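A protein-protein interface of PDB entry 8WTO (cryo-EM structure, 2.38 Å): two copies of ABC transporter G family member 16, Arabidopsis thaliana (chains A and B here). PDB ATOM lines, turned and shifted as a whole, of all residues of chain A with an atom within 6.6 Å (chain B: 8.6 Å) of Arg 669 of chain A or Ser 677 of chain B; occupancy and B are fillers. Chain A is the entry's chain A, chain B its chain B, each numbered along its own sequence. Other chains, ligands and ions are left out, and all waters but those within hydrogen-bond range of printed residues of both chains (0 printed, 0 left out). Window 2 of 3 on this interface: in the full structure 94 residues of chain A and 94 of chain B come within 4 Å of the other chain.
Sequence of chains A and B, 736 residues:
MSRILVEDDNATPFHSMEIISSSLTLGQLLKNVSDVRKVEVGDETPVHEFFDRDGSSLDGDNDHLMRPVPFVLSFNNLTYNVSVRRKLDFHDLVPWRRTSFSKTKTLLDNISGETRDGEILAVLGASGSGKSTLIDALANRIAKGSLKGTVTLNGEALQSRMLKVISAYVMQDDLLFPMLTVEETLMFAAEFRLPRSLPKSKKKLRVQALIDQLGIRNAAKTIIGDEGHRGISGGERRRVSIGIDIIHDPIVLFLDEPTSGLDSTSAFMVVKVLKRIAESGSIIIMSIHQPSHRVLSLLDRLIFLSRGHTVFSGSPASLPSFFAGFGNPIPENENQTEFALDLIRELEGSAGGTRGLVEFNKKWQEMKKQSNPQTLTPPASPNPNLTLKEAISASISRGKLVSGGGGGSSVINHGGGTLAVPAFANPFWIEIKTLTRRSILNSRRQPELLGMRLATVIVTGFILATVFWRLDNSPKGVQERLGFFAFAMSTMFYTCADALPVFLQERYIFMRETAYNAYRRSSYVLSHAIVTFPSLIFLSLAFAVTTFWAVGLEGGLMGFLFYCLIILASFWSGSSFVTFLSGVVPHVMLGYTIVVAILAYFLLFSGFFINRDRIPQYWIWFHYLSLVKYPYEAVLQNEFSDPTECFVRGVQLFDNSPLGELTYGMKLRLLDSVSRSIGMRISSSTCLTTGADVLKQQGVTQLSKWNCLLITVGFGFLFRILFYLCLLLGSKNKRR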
ATOM      1  N   TYR A 664      13.297   1.750  15.949  1.00  0.00           N
ATOM      2  CA  TYR A 664      14.432   1.150  16.644  1.00  0.00           C
ATOM      3  C   TYR A 664      15.369   2.212  17.202  1.00  0.00           C
ATOM      4  O   TYR A 664      15.872   2.072  18.322  1.00  0.00           O
ATOM      5  CB  TYR A 664      15.193   0.214  15.705  1.00  0.00           C
ATOM      6  CG  TYR A 664      16.532  -0.244  16.241  1.00  0.00           C
ATOM      7  CD1 TYR A 664      17.723   0.239  15.705  1.00  0.00           C
ATOM      8  CD2 TYR A 664      16.606  -1.163  17.279  1.00  0.00           C
ATOM      9  CE1 TYR A 664      18.947  -0.178  16.196  1.00  0.00           C
ATOM     10  CE2 TYR A 664      17.825  -1.589  17.772  1.00  0.00           C
ATOM     11  CZ  TYR A 664      18.990  -1.093  17.228  1.00  0.00           C
ATOM     12  OH  TYR A 664      20.205  -1.514  17.718  1.00  0.00           O
ATOM     13  N   GLY A 665      15.611   3.280  16.441  1.00  0.00           N
ATOM     14  CA  GLY A 665      16.506   4.324  16.906  1.00  0.00           C
ATOM     15  C   GLY A 665      15.934   5.150  18.038  1.00  0.00           C
ATOM     16  O   GLY A 665      16.683   5.693  18.854  1.00  0.00           O
ATOM     17  N   MET A 666      14.611   5.254  18.115  1.00  0.00           N
ATOM     18  CA  MET A 666      13.992   6.013  19.190  1.00  0.00           C
ATOM     19  C   MET A 666      13.754   5.147  20.425  1.00  0.00           C
ATOM     20  O   MET A 666      13.603   5.681  21.530  1.00  0.00           O
ATOM     21  CB  MET A 666      12.696   6.660  18.675  1.00  0.00           C
ATOM     22  CG  MET A 666      12.006   7.651  19.607  1.00  0.00           C
ATOM     23  SD  MET A 666      10.464   7.037  20.287  1.00  0.00           S
ATOM     24  CE  MET A 666       9.489   6.879  18.793  1.00  0.00           C
ATOM     25  N   LYS A 667      13.761   3.820  20.270  1.00  0.00           N
ATOM     26  CA  LYS A 667      13.841   2.954  21.441  1.00  0.00           C
ATOM     27  C   LYS A 667      15.200   3.067  22.117  1.00  0.00           C
ATOM     28  O   LYS A 667      15.291   2.944  23.341  1.00  0.00           O
ATOM     29  CB  LYS A 667      13.553   1.504  21.058  1.00  0.00           C
ATOM     30  CG  LYS A 667      12.078   1.179  20.966  1.00  0.00           C
ATOM     31  CD  LYS A 667      11.842  -0.299  20.741  1.00  0.00           C
ATOM     32  CE  LYS A 667      12.349  -0.739  19.384  1.00  0.00           C
ATOM     33  NZ  LYS A 667      11.761  -2.045  18.979  1.00  0.00           N
ATOM     34  N   LEU A 668      16.261   3.313  21.343  1.00  0.00           N
ATOM     35  CA  LEU A 668      17.557   3.633  21.933  1.00  0.00           C
ATOM     36  C   LEU A 668      17.588   5.021  22.557  1.00  0.00           C
ATOM     37  O   LEU A 668      18.421   5.267  23.435  1.00  0.00           O
ATOM     38  CB  LEU A 668      18.670   3.512  20.893  1.00  0.00           C
ATOM     39  CG  LEU A 668      19.367   2.157  20.734  1.00  0.00           C
ATOM     40  CD1 LEU A 668      18.485   1.112  20.091  1.00  0.00           C
ATOM     41  CD2 LEU A 668      20.651   2.329  19.938  1.00  0.00           C
ATOM     42  N   ARG A 669      16.719   5.931  22.115  1.00  0.00           N
ATOM     43  CA  ARG A 669      16.577   7.211  22.801  1.00  0.00           C
ATOM     44  C   ARG A 669      15.984   7.024  24.190  1.00  0.00           C
ATOM     45  O   ARG A 669      16.368   7.724  25.134  1.00  0.00           O
ATOM     46  CB  ARG A 669      15.706   8.160  21.981  1.00  0.00           C
ATOM     47  CG  ARG A 669      16.333   8.656  20.696  1.00  0.00           C
ATOM     48  CD  ARG A 669      15.332   9.468  19.893  1.00  0.00           C
ATOM     49  NE  ARG A 669      14.856  10.634  20.630  1.00  0.00           N
ATOM     50  CZ  ARG A 669      15.460  11.818  20.632  1.00  0.00           C
ATOM     51  NH1 ARG A 669      14.950  12.820  21.332  1.00  0.00           N
ATOM     52  NH2 ARG A 669      16.573  11.998  19.935  1.00  0.00           N
ATOM     53  N   LEU A 670      15.045   6.087  24.332  1.00  0.00           N
ATOM     54  CA  LEU A 670      14.458   5.821  25.638  1.00  0.00           C
ATOM     55  C   LEU A 670      15.407   5.057  26.546  1.00  0.00           C
ATOM     56  O   LEU A 670      15.330   5.207  27.767  1.00  0.00           O
ATOM     57  CB  LEU A 670      13.160   5.038  25.495  1.00  0.00           C
ATOM     58  CG  LEU A 670      11.950   5.818  25.002  1.00  0.00           C
ATOM     59  CD1 LEU A 670      10.912   4.850  24.525  1.00  0.00           C
ATOM     60  CD2 LEU A 670      11.407   6.707  26.083  1.00  0.00           C
ATOM     61  N   LEU A 671      16.285   4.231  25.973  1.00  0.00           N
ATOM     62  CA  LEU A 671      17.259   3.489  26.768  1.00  0.00           C
ATOM     63  C   LEU A 671      18.245   4.427  27.445  1.00  0.00           C
ATOM     64  O   LEU A 671      18.613   4.219  28.607  1.00  0.00           O
ATOM     65  CB  LEU A 671      18.006   2.507  25.876  1.00  0.00           C
ATOM     66  CG  LEU A 671      17.240   1.274  25.416  1.00  0.00           C
ATOM     67  CD1 LEU A 671      18.073   0.563  24.378  1.00  0.00           C
ATOM     68  CD2 LEU A 671      16.921   0.366  26.583  1.00  0.00           C
ATOM     69  N   ASP A 672      18.686   5.464  26.730  1.00  0.00           N
ATOM     70  CA  ASP A 672      19.508   6.494  27.349  1.00  0.00           C
ATOM     71  C   ASP A 672      18.715   7.299  28.365  1.00  0.00           C
ATOM     72  O   ASP A 672      19.257   7.679  29.406  1.00  0.00           O
ATOM     73  CB  ASP A 672      20.085   7.422  26.281  1.00  0.00           C
ATOM     74  CG  ASP A 672      21.110   6.735  25.402  1.00  0.00           C
ATOM     75  OD1 ASP A 672      21.791   5.809  25.891  1.00  0.00           O
ATOM     76  OD2 ASP A 672      21.232   7.117  24.219  1.00  0.00           O
ATOM     77  N   SER A 673      17.431   7.544  28.092  1.00  0.00           N
ATOM     78  CA  SER A 673      16.621   8.396  28.953  1.00  0.00           C
ATOM     79  C   SER A 673      16.229   7.696  30.250  1.00  0.00           C
ATOM     80  O   SER A 673      16.196   8.332  31.308  1.00  0.00           O
ATOM     81  CB  SER A 673      15.375   8.864  28.202  1.00  0.00           C
ATOM     82  OG  SER A 673      15.725   9.656  27.081  1.00  0.00           O
ATOM     83  N   VAL A 674      15.927   6.396  30.199  1.00  0.00           N
ATOM     84  CA  VAL A 674      15.645   5.674  31.438  1.00  0.00           C
ATOM     85  C   VAL A 674      16.921   5.301  32.181  1.00  0.00           C
ATOM     86  O   VAL A 674      16.849   4.861  33.335  1.00  0.00           O
ATOM     87  CB  VAL A 674      14.798   4.411  31.202  1.00  0.00           C
ATOM     88  CG1 VAL A 674      13.519   4.755  30.460  1.00  0.00           C
ATOM     89  CG2 VAL A 674      15.595   3.341  30.475  1.00  0.00           C
ATOM     90  N   LEU B 670      10.739   8.894  35.505  1.00  0.00           N
ATOM     91  CA  LEU B 670      10.742   8.258  34.196  1.00  0.00           C
ATOM     92  C   LEU B 670       9.666   8.814  33.278  1.00  0.00           C
ATOM     93  O   LEU B 670       9.877   8.867  32.066  1.00  0.00           O
ATOM     94  CB  LEU B 670      10.558   6.749  34.328  1.00  0.00           C
ATOM     95  CG  LEU B 670      11.713   5.936  34.892  1.00  0.00           C
ATOM     96  CD1 LEU B 670      11.289   4.500  34.987  1.00  0.00           C
ATOM     97  CD2 LEU B 670      12.903   6.069  33.985  1.00  0.00           C
ATOM     98  N   LEU B 671       8.529   9.240  33.832  1.00  0.00           N
ATOM     99  CA  LEU B 671       7.437   9.751  33.007  1.00  0.00           C
ATOM    100  C   LEU B 671       7.815  11.063  32.340  1.00  0.00           C
ATOM    101  O   LEU B 671       7.468  11.299  31.177  1.00  0.00           O
ATOM    102  CB  LEU B 671       6.191   9.943  33.859  1.00  0.00           C
ATOM    103  CG  LEU B 671       5.503   8.645  34.252  1.00  0.00           C
ATOM    104  CD1 LEU B 671       4.754   8.856  35.551  1.00  0.00           C
ATOM    105  CD2 LEU B 671       4.598   8.179  33.144  1.00  0.00           C
ATOM    106  N   ASP B 672       8.522  11.926  33.068  1.00  0.00           N
ATOM    107  CA  ASP B 672       9.086  13.121  32.459  1.00  0.00           C
ATOM    108  C   ASP B 672      10.192  12.756  31.479  1.00  0.00           C
ATOM    109  O   ASP B 672      10.336  13.407  30.441  1.00  0.00           O
ATOM    110  CB  ASP B 672       9.610  14.053  33.553  1.00  0.00           C
ATOM    111  CG  ASP B 672       9.815  15.479  33.073  1.00  0.00           C
ATOM    112  OD1 ASP B 672       9.539  15.778  31.892  1.00  0.00           O
ATOM    113  OD2 ASP B 672      10.250  16.314  33.894  1.00  0.00           O
ATOM    114  N   SER B 673      10.953  11.700  31.775  1.00  0.00           N
ATOM    115  CA  SER B 673      12.065  11.299  30.919  1.00  0.00           C
ATOM    116  C   SER B 673      11.590  10.610  29.645  1.00  0.00           C
ATOM    117  O   SER B 673      12.195  10.792  28.584  1.00  0.00           O
ATOM    118  CB  SER B 673      13.020  10.391  31.691  1.00  0.00           C
ATOM    119  OG  SER B 673      13.557  11.056  32.821  1.00  0.00           O
ATOM    120  N   VAL B 674      10.519   9.811  29.720  1.00  0.00           N
ATOM    121  CA  VAL B 674       9.949   9.237  28.499  1.00  0.00           C
ATOM    122  C   VAL B 674       9.084  10.232  27.744  1.00  0.00           C
ATOM    123  O   VAL B 674       8.691   9.955  26.604  1.00  0.00           O
ATOM    124  CB  VAL B 674       9.111   7.970  28.759  1.00  0.00           C
ATOM    125  CG1 VAL B 674       9.933   6.914  29.483  1.00  0.00           C
ATOM    126  CG2 VAL B 674       7.838   8.298  29.522  1.00  0.00           C
ATOM    127  N   SER B 675       8.774  11.382  28.345  1.00  0.00           N
ATOM    128  CA  SER B 675       8.128  12.461  27.609  1.00  0.00           C
ATOM    129  C   SER B 675       9.119  13.203  26.723  1.00  0.00           C
ATOM    130  O   SER B 675       8.720  13.798  25.716  1.00  0.00           O
ATOM    131  CB  SER B 675       7.463  13.434  28.580  1.00  0.00           C
ATOM    132  OG  SER B 675       6.442  12.794  29.323  1.00  0.00           O
ATOM    133  N   ARG B 676      10.405  13.175  27.082  1.00  0.00           N
ATOM    134  CA  ARG B 676      11.428  13.889  26.331  1.00  0.00           C
ATOM    135  C   ARG B 676      11.712  13.262  24.976  1.00  0.00           C
ATOM    136  O   ARG B 676      12.108  13.975  24.049  1.00  0.00           O
ATOM    137  CB  ARG B 676      12.735  13.926  27.122  1.00  0.00           C
ATOM    138  CG  ARG B 676      12.659  14.582  28.481  1.00  0.00           C
ATOM    139  CD  ARG B 676      12.526  16.087  28.396  1.00  0.00           C
ATOM    140  NE  ARG B 676      12.493  16.678  29.730  1.00  0.00           N
ATOM    141  CZ  ARG B 676      13.577  17.022  30.421  1.00  0.00           C
ATOM    142  NH1 ARG B 676      14.784  16.828  29.906  1.00  0.00           N
ATOM    143  NH2 ARG B 676      13.455  17.553  31.630  1.00  0.00           N
ATOM    144  N   SER B 677      11.520  11.949  24.838  1.00  0.00           N
ATOM    145  CA  SER B 677      12.031  11.226  23.685  1.00  0.00           C
ATOM    146  C   SER B 677      10.979  10.863  22.651  1.00  0.00           C
ATOM    147  O   SER B 677      11.345  10.527  21.522  1.00  0.00           O
ATOM    148  CB  SER B 677      12.737   9.942  24.140  1.00  0.00           C
ATOM    149  OG  SER B 677      13.570  10.201  25.256  1.00  0.00           O
ATOM    150  N   ILE B 678       9.696  10.916  22.998  1.00  0.00           N
ATOM    151  CA  ILE B 678       8.635  10.536  22.070  1.00  0.00           C
ATOM    152  C   ILE B 678       7.815  11.722  21.597  1.00  0.00           C
ATOM    153  O   ILE B 678       7.050  11.577  20.628  1.00  0.00           O
ATOM    154  CB  ILE B 678       7.705   9.465  22.679  1.00  0.00           C
ATOM    155  CG1 ILE B 678       6.860  10.060  23.802  1.00  0.00           C
ATOM    156  CG2 ILE B 678       8.512   8.297  23.212  1.00  0.00           C
ATOM    157  CD1 ILE B 678       5.757   9.145  24.275  1.00  0.00           C
ATOM    158  N   GLY B 679       7.945  12.881  22.231  1.00  0.00           N
ATOM    159  CA  GLY B 679       7.162  14.056  21.894  1.00  0.00           C
ATOM    160  C   GLY B 679       5.854  14.176  22.645  1.00  0.00           C
ATOM    161  O   GLY B 679       5.458  15.278  23.028  1.00  0.00           O
ATOM    162  N   MET B 680       5.170  13.056  22.863  1.00  0.00           N
ATOM    163  CA  MET B 680       3.902  13.067  23.576  1.00  0.00           C
ATOM    164  C   MET B 680       4.140  13.271  25.066  1.00  0.00           C
ATOM    165  O   MET B 680       5.023  12.642  25.655  1.00  0.00           O
ATOM    166  CB  MET B 680       3.141  11.765  23.329  1.00  0.00           C
ATOM    167  CG  MET B 680       1.757  11.732  23.952  1.00  0.00           C
ATOM    168  SD  MET B 680       0.656  12.980  23.262  1.00  0.00           S
ATOM    169  CE  MET B 680      -0.485  13.212  24.622  1.00  0.00           C
ATOM    170  N   ARG B 681       3.359  14.160  25.670  1.00  0.00           N
ATOM    171  CA  ARG B 681       3.473  14.459  27.092  1.00  0.00           C
ATOM    172  C   ARG B 681       2.620  13.470  27.874  1.00  0.00           C
ATOM    173  O   ARG B 681       1.392  13.455  27.743  1.00  0.00           O
ATOM    174  CB  ARG B 681       3.047  15.894  27.382  1.00  0.00           C
ATOM    175  CG  ARG B 681       3.149  16.268  28.846  1.00  0.00           C
ATOM    176  CD  ARG B 681       4.562  16.072  29.364  1.00  0.00           C
ATOM    177  NE  ARG B 681       4.667  16.357  30.790  1.00  0.00           N
ATOM    178  CZ  ARG B 681       5.808  16.344  31.469  1.00  0.00           C
ATOM    179  NH1 ARG B 681       5.815  16.618  32.766  1.00  0.00           N
ATOM    180  NH2 ARG B 681       6.945  16.056  30.852  1.00  0.00           N
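The side-chain hydroxyl of Ser 673 of chain A sits at hydrogen-bond distance from the backbone carbonyl oxygen of Arg 669 of chain A.
Arg 669 of chain A touches just one residue of chain B: Ser 677 (3.6 Å).
Of the printed residues of chain A, Ser 677 of chain B touches Met 666 (3.5 Å), Arg 669 (3.6 Å) and Ser 673 (2.9 Å).
Printed residues of chain B within 4 Å of Ser 673 of chain A: Ser 673 (3.7 Å) and Ser 677 (2.9 Å).
Of the printed residues of chain A, Ile 678 of chain B touches Met 666.
Of the printed residues of chain A, Leu 670 of chain B touches Val 674.
Of the printed residues of chain A, Val 674 of chain B touches Leu 670 (3.7 Å).
Printed residues of chain B within 4 Å of Met 666 of chain A: Ser 677 and Ile 678.
Asp 672 of chain B touches none of the printed residues of chain A.
Gly 665 of chain A touches none of the printed residues of chain B.
Among the printed residues, merely in contact across the chains: Met 666 of chain A with Ser 677 of chain B (3.5 Å), Arg 669 of chain A with Ser 677 of chain B (3.6 Å), Leu 670 of chain A with Val 674 of chain B (3.7 Å), Met 666 of chain A with Ile 678 of chain B (3.7 Å), Ser 673 of chain A with Ser 673 of chain B (3.7 Å) and Val 674 of chain A with Leu 670 of chain B (3.8 Å).
The side-chain hydroxyl of Ser 673 of chain A lies within hydrogen-bond range of the side-chain hydroxyl of Ser 677 of chain B (2.9 Å).
Hydrophobic or aromatic side chains of chain A within 4 Å of the printed part of chain B: Met 666, Leu 670 and Val 674.
Of the 12 printed residues of chain B, 5 touch a printed residue of chain A.
Hydrophobic or aromatic side chains of chain B that line the printed part of chain A: Leu 670, Val 674 and Ile 678.
Among the printed residues, 7 pairs touch across the chains.
Leu 670 of chain A touches Val 674 of chain B, and with the chains exchanged Val 674 of chain A touches Leu 670 of chain B.
Ser 673 of chain B touches its own counterpart, Ser 673 of chain A.
Positions printed for both chains: 670, 671, 672, 673 and 674.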
